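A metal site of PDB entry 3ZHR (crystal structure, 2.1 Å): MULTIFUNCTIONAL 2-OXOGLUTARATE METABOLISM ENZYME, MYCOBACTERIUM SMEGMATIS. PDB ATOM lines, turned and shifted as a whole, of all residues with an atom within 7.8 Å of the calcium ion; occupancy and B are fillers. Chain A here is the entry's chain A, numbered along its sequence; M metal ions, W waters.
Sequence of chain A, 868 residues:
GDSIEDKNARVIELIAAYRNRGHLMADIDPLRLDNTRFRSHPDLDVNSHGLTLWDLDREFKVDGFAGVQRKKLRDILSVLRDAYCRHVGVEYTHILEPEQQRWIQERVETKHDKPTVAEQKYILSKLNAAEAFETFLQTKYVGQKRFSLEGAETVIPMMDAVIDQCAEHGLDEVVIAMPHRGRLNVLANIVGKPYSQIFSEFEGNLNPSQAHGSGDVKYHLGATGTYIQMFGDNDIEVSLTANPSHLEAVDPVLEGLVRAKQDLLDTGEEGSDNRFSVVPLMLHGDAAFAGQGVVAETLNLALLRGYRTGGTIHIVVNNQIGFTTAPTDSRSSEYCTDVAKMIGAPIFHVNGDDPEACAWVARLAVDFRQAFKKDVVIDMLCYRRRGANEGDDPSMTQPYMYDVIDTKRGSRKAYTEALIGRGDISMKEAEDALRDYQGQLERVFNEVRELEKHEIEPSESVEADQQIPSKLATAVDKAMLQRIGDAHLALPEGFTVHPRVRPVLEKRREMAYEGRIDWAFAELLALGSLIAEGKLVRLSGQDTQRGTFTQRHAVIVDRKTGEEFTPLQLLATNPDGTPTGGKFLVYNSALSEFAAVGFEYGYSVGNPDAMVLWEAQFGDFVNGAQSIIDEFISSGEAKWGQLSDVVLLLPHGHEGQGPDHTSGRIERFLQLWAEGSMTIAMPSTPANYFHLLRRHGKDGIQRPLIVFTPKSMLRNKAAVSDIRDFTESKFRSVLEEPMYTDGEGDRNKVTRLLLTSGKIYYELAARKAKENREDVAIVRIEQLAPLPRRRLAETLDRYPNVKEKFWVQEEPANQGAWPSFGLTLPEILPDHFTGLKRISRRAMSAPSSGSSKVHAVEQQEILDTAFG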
ATOM      1  N   LYS A 535      24.934  12.423  -5.433  1.00  0.00           N
ATOM      2  CA  LYS A 535      24.857  12.316  -3.971  1.00  0.00           C
ATOM      3  C   LYS A 535      25.708  11.182  -3.392  1.00  0.00           C
ATOM      4  O   LYS A 535      25.799  10.098  -3.970  1.00  0.00           O
ATOM      5  CB  LYS A 535      23.409  12.118  -3.511  1.00  0.00           C
ATOM      6  CG  LYS A 535      23.136  12.751  -2.162  1.00  0.00           C
ATOM      7  CD  LYS A 535      21.681  12.781  -1.841  1.00  0.00           C
ATOM      8  CE  LYS A 535      21.458  13.345  -0.457  1.00  0.00           C
ATOM      9  NZ  LYS A 535      21.531  14.823  -0.439  1.00  0.00           N
ATOM     10  N   PRO A 608      25.912  17.165   5.894  1.00  0.00           N
ATOM     11  CA  PRO A 608      24.469  17.335   5.640  1.00  0.00           C
ATOM     12  C   PRO A 608      24.020  16.983   4.211  1.00  0.00           C
ATOM     13  O   PRO A 608      22.829  16.771   3.993  1.00  0.00           O
ATOM     14  CB  PRO A 608      24.248  18.829   5.915  1.00  0.00           C
ATOM     15  CG  PRO A 608      25.416  19.259   6.778  1.00  0.00           C
ATOM     16  CD  PRO A 608      26.557  18.434   6.290  1.00  0.00           C
ATOM     17  N   ALA A 610      25.040  14.296   2.554  1.00  0.00           N
ATOM     18  CA  ALA A 610      25.039  12.854   2.408  1.00  0.00           C
ATOM     19  C   ALA A 610      23.640  12.271   2.690  1.00  0.00           C
ATOM     20  O   ALA A 610      22.882  12.818   3.492  1.00  0.00           O
ATOM     21  CB  ALA A 610      26.061  12.237   3.359  1.00  0.00           C
ATOM     22  N   MET A 611      23.318  11.170   1.995  1.00  0.00           N
ATOM     23  CA  MET A 611      22.130  10.350   2.246  1.00  0.00           C
ATOM     24  C   MET A 611      22.648   9.257   3.188  1.00  0.00           C
ATOM     25  O   MET A 611      23.529   8.497   2.792  1.00  0.00           O
ATOM     26  CB  MET A 611      21.554   9.807   0.920  1.00  0.00           C
ATOM     27  CG  MET A 611      20.332   8.900   1.107  1.00  0.00           C
ATOM     28  SD  MET A 611      18.766   9.785   1.318  1.00  0.00           S
ATOM     29  CE  MET A 611      17.647   8.469   1.206  1.00  0.00           C
ATOM     30  N   SER A 644      20.128  16.849  11.687  1.00  0.00           N
ATOM     31  CA  SER A 644      20.481  15.554  11.146  1.00  0.00           C
ATOM     32  C   SER A 644      19.448  15.136  10.115  1.00  0.00           C
ATOM     33  O   SER A 644      18.266  15.404  10.325  1.00  0.00           O
ATOM     34  CB  SER A 644      20.531  14.520  12.266  1.00  0.00           C
ATOM     35  OG  SER A 644      20.985  13.253  11.798  1.00  0.00           O
ATOM     36  N   ASP A 645      19.871  14.444   9.058  1.00  0.00           N
ATOM     37  CA  ASP A 645      18.996  13.897   8.009  1.00  0.00           C
ATOM     38  C   ASP A 645      19.100  12.377   8.012  1.00  0.00           C
ATOM     39  O   ASP A 645      18.795  11.733   7.007  1.00  0.00           O
ATOM     40  CB  ASP A 645      19.373  14.495   6.622  1.00  0.00           C
ATOM     41  CG  ASP A 645      18.188  14.699   5.686  1.00  0.00           C
ATOM     42  OD1 ASP A 645      17.087  15.036   6.185  1.00  0.00           O
ATOM     43  OD2 ASP A 645      18.385  14.600   4.454  1.00  0.00           O
ATOM     44  N   VAL A 646      19.533  11.782   9.136  1.00  0.00           N
ATOM     45  CA  VAL A 646      19.692  10.333   9.274  1.00  0.00           C
ATOM     46  C   VAL A 646      18.375   9.583   9.037  1.00  0.00           C
ATOM     47  O   VAL A 646      17.295  10.040   9.429  1.00  0.00           O
ATOM     48  CB  VAL A 646      20.350   9.913  10.635  1.00  0.00           C
ATOM     49  CG1 VAL A 646      19.408  10.066  11.830  1.00  0.00           C
ATOM     50  CG2 VAL A 646      20.911   8.499  10.552  1.00  0.00           C
ATOM     51  N   VAL A 647      18.453   8.463   8.340  1.00  0.00           N
ATOM     52  CA  VAL A 647      17.326   7.566   8.085  1.00  0.00           C
ATOM     53  C   VAL A 647      17.507   6.327   8.942  1.00  0.00           C
ATOM     54  O   VAL A 647      18.596   5.739   8.929  1.00  0.00           O
ATOM     55  CB  VAL A 647      17.176   7.168   6.582  1.00  0.00           C
ATOM     56  CG1 VAL A 647      15.914   6.324   6.346  1.00  0.00           C
ATOM     57  CG2 VAL A 647      17.190   8.382   5.657  1.00  0.00           C
ATOM     58  N   LEU A 693      12.316   8.011  -0.177  1.00  0.00           N
ATOM     59  CA  LEU A 693      13.781   8.158  -0.027  1.00  0.00           C
ATOM     60  C   LEU A 693      14.316   9.294  -0.892  1.00  0.00           C
ATOM     61  O   LEU A 693      15.171  10.072  -0.447  1.00  0.00           O
ATOM     62  CB  LEU A 693      14.524   6.862  -0.373  1.00  0.00           C
ATOM     63  CG  LEU A 693      14.295   5.634   0.506  1.00  0.00           C
ATOM     64  CD1 LEU A 693      15.048   4.430  -0.058  1.00  0.00           C
ATOM     65  CD2 LEU A 693      14.717   5.889   1.964  1.00  0.00           C
ATOM     66  N   ARG A 694      13.812   9.413  -2.131  1.00  0.00           N
ATOM     67  CA  ARG A 694      14.250  10.478  -3.029  1.00  0.00           C
ATOM     68  C   ARG A 694      13.820  11.859  -2.493  1.00  0.00           C
ATOM     69  O   ARG A 694      14.625  12.788  -2.527  1.00  0.00           O
ATOM     70  CB  ARG A 694      13.771  10.234  -4.449  1.00  0.00           C
ATOM     71  CG  ARG A 694      14.647   9.165  -5.103  1.00  0.00           C
ATOM     72  CD  ARG A 694      14.405   8.979  -6.579  1.00  0.00           C
ATOM     73  NE  ARG A 694      14.399  10.214  -7.368  1.00  0.00           N
ATOM     74  CZ  ARG A 694      15.474  10.868  -7.781  1.00  0.00           C
ATOM     75  NH1 ARG A 694      16.684  10.433  -7.451  1.00  0.00           N
ATOM     76  NH2 ARG A 694      15.351  11.954  -8.522  1.00  0.00           N
ATOM     77  N   ARG A 695      12.574  11.976  -1.944  1.00  0.00           N
ATOM     78  CA  ARG A 695      12.107  13.246  -1.365  1.00  0.00           C
ATOM     79  C   ARG A 695      13.001  13.624  -0.195  1.00  0.00           C
ATOM     80  O   ARG A 695      13.434  14.764  -0.111  1.00  0.00           O
ATOM     81  CB  ARG A 695      10.621  13.144  -0.939  1.00  0.00           C
ATOM     82  CG  ARG A 695      10.070  14.426  -0.278  1.00  0.00           C
ATOM     83  CD  ARG A 695       8.645  14.257   0.248  1.00  0.00           C
ATOM     84  NE  ARG A 695       8.573  13.362   1.415  1.00  0.00           N
ATOM     85  CZ  ARG A 695       7.511  13.220   2.196  1.00  0.00           C
ATOM     86  NH1 ARG A 695       6.405  13.908   1.972  1.00  0.00           N
ATOM     87  NH2 ARG A 695       7.551  12.376   3.229  1.00  0.00           N
ATOM     88  N   HIS A 696      13.329  12.644   0.672  1.00  0.00           N
ATOM     89  CA  HIS A 696      14.167  12.833   1.852  1.00  0.00           C
ATOM     90  C   HIS A 696      15.563  13.333   1.497  1.00  0.00           C
ATOM     91  O   HIS A 696      16.075  14.211   2.179  1.00  0.00           O
ATOM     92  CB  HIS A 696      14.261  11.537   2.662  1.00  0.00           C
ATOM     93  CG  HIS A 696      15.121  11.661   3.875  1.00  0.00           C
ATOM     94  ND1 HIS A 696      14.671  12.317   5.012  1.00  0.00           N
ATOM     95  CD2 HIS A 696      16.410  11.289   4.063  1.00  0.00           C
ATOM     96  CE1 HIS A 696      15.679  12.260   5.879  1.00  0.00           C
ATOM     97  NE2 HIS A 696      16.750  11.667   5.340  1.00  0.00           N
ATOM     98  N   GLY A 697      16.160  12.772   0.460  1.00  0.00           N
ATOM     99  CA  GLY A 697      17.510  13.157   0.040  1.00  0.00           C
ATOM    100  C   GLY A 697      17.599  14.430  -0.768  1.00  0.00           C
ATOM    101  O   GLY A 697      18.657  15.039  -0.826  1.00  0.00           O
ATOM    102  N   LYS A 698      16.477  14.853  -1.391  1.00  0.00           N
ATOM    103  CA  LYS A 698      16.490  16.039  -2.274  1.00  0.00           C
ATOM    104  C   LYS A 698      15.708  17.266  -1.743  1.00  0.00           C
ATOM    105  O   LYS A 698      15.789  18.317  -2.390  1.00  0.00           O
ATOM    106  CB  LYS A 698      15.897  15.663  -3.650  1.00  0.00           C
ATOM    107  CG  LYS A 698      16.659  14.557  -4.410  1.00  0.00           C
ATOM    108  CD  LYS A 698      15.866  14.016  -5.615  1.00  0.00           C
ATOM    109  CE  LYS A 698      15.819  14.967  -6.795  1.00  0.00           C
ATOM    110  NZ  LYS A 698      17.172  15.186  -7.390  1.00  0.00           N
ATOM    111  N   ASP A 699      14.977  17.164  -0.618  1.00  0.00           N
ATOM    112  CA  ASP A 699      14.127  18.254  -0.099  1.00  0.00           C
ATOM    113  C   ASP A 699      14.892  19.464   0.509  1.00  0.00           C
ATOM    114  O   ASP A 699      14.249  20.453   0.878  1.00  0.00           O
ATOM    115  CB  ASP A 699      13.112  17.709   0.931  1.00  0.00           C
ATOM    116  CG  ASP A 699      13.706  17.010   2.152  1.00  0.00           C
ATOM    117  OD1 ASP A 699      14.951  17.114   2.357  1.00  0.00           O
ATOM    118  OD2 ASP A 699      12.936  16.365   2.901  1.00  0.00           O
ATOM    119  N   GLY A 700      16.208  19.382   0.649  1.00  0.00           N
ATOM    120  CA  GLY A 700      17.006  20.482   1.207  1.00  0.00           C
ATOM    121  C   GLY A 700      16.752  20.787   2.680  1.00  0.00           C
ATOM    122  O   GLY A 700      17.120  21.867   3.153  1.00  0.00           O
ATOM    123  N   ILE A 701      16.095  19.840   3.389  1.00  0.00           N
ATOM    124  CA  ILE A 701      15.707  19.904   4.803  1.00  0.00           C
ATOM    125  C   ILE A 701      16.536  18.828   5.566  1.00  0.00           C
ATOM    126  O   ILE A 701      16.680  17.714   5.082  1.00  0.00           O
ATOM    127  CB  ILE A 701      14.148  19.687   4.915  1.00  0.00           C
ATOM    128  CG1 ILE A 701      13.367  20.948   4.499  1.00  0.00           C
ATOM    129  CG2 ILE A 701      13.689  19.196   6.306  1.00  0.00           C
ATOM    130  CD1 ILE A 701      11.803  20.753   4.307  1.00  0.00           C
ATOM    131  N   GLN A 702      17.065  19.183   6.745  1.00  0.00           N
ATOM    132  CA  GLN A 702      17.812  18.235   7.574  1.00  0.00           C
ATOM    133  C   GLN A 702      16.874  17.784   8.686  1.00  0.00           C
ATOM    134  O   GLN A 702      16.680  18.486   9.678  1.00  0.00           O
ATOM    135  CB  GLN A 702      19.121  18.845   8.104  1.00  0.00           C
ATOM    136  CG  GLN A 702      20.042  19.410   7.010  1.00  0.00           C
ATOM    137  CD  GLN A 702      20.352  18.404   5.937  1.00  0.00           C
ATOM    138  OE1 GLN A 702      20.995  17.389   6.169  1.00  0.00           O
ATOM    139  NE2 GLN A 702      19.876  18.645   4.715  1.00  0.00           N
ATOM    140  N   ARG A 703      16.244  16.626   8.475  1.00  0.00           N
ATOM    141  CA  ARG A 703      15.276  16.070   9.426  1.00  0.00           C
ATOM    142  C   ARG A 703      15.303  14.554   9.406  1.00  0.00           C
ATOM    143  O   ARG A 703      15.163  13.965   8.342  1.00  0.00           O
ATOM    144  CB  ARG A 703      13.871  16.573   9.066  1.00  0.00           C
ATOM    145  CG  ARG A 703      12.799  16.221  10.083  1.00  0.00           C
ATOM    146  CD  ARG A 703      11.492  16.922   9.771  1.00  0.00           C
ATOM    147  NE  ARG A 703      11.663  18.368   9.851  1.00  0.00           N
ATOM    148  CZ  ARG A 703      10.860  19.259   9.295  1.00  0.00           C
ATOM    149  NH1 ARG A 703       9.797  18.870   8.590  1.00  0.00           N
ATOM    150  NH2 ARG A 703      11.110  20.553   9.417  1.00  0.00           N
ATOM    151  N   PRO A 704      15.429  13.871  10.567  1.00  0.00           N
ATOM    152  CA  PRO A 704      15.458  12.401  10.543  1.00  0.00           C
ATOM    153  C   PRO A 704      14.196  11.760   9.982  1.00  0.00           C
ATOM    154  O   PRO A 704      13.099  12.300  10.098  1.00  0.00           O
ATOM    155  CB  PRO A 704      15.664  12.027  12.010  1.00  0.00           C
ATOM    156  CG  PRO A 704      16.313  13.270  12.614  1.00  0.00           C
ATOM    157  CD  PRO A 704      15.631  14.391  11.931  1.00  0.00           C
ATOM    158  N   LEU A 705      14.388  10.637   9.290  1.00  0.00           N
ATOM    159  CA  LEU A 705      13.299   9.867   8.695  1.00  0.00           C
ATOM    160  C   LEU A 705      13.294   8.487   9.346  1.00  0.00           C
ATOM    161  O   LEU A 705      14.337   7.822   9.386  1.00  0.00           O
ATOM    162  CB  LEU A 705      13.432   9.784   7.159  1.00  0.00           C
ATOM    163  CG  LEU A 705      12.495   8.803   6.402  1.00  0.00           C
ATOM    164  CD1 LEU A 705      11.010   9.224   6.497  1.00  0.00           C
ATOM    165  CD2 LEU A 705      12.897   8.681   4.944  1.00  0.00           C
HETATM  166 CA    CA M   1      16.465  15.777   3.817  1.00  0.00          CA
HETATM  167  O   HOH W   1      14.531  15.447   4.756  1.00  0.00           O
HETATM  168  O   HOH W   2      18.268  16.786   2.479  1.00  0.00           O
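OD1 of Asp 645 sits close to N of Arg 703 (2.9 Å).
Water W1 bridges OD2 of Asp 699 (2.6 Å) and ND1 of His 696 (3.1 Å).
Water W1 binds the calcium ion.
The calcium ion is bound by O of His 696, at 2.3 Å.
O of Ile 701 is bound to the calcium ion (2.3 Å).
OD2 of Asp 645 is bound to the calcium ion.
Water W2 is bound to the calcium ion (2.5 Å).
OD1 of Asp 699 binds the calcium ion, 2.5 Å away.
OD1 of Asp 645 is bound to the calcium ion, 2.6 Å away.
The nearest printed residue that does not touch the calcium ion is Gly 697 (4.5 Å).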
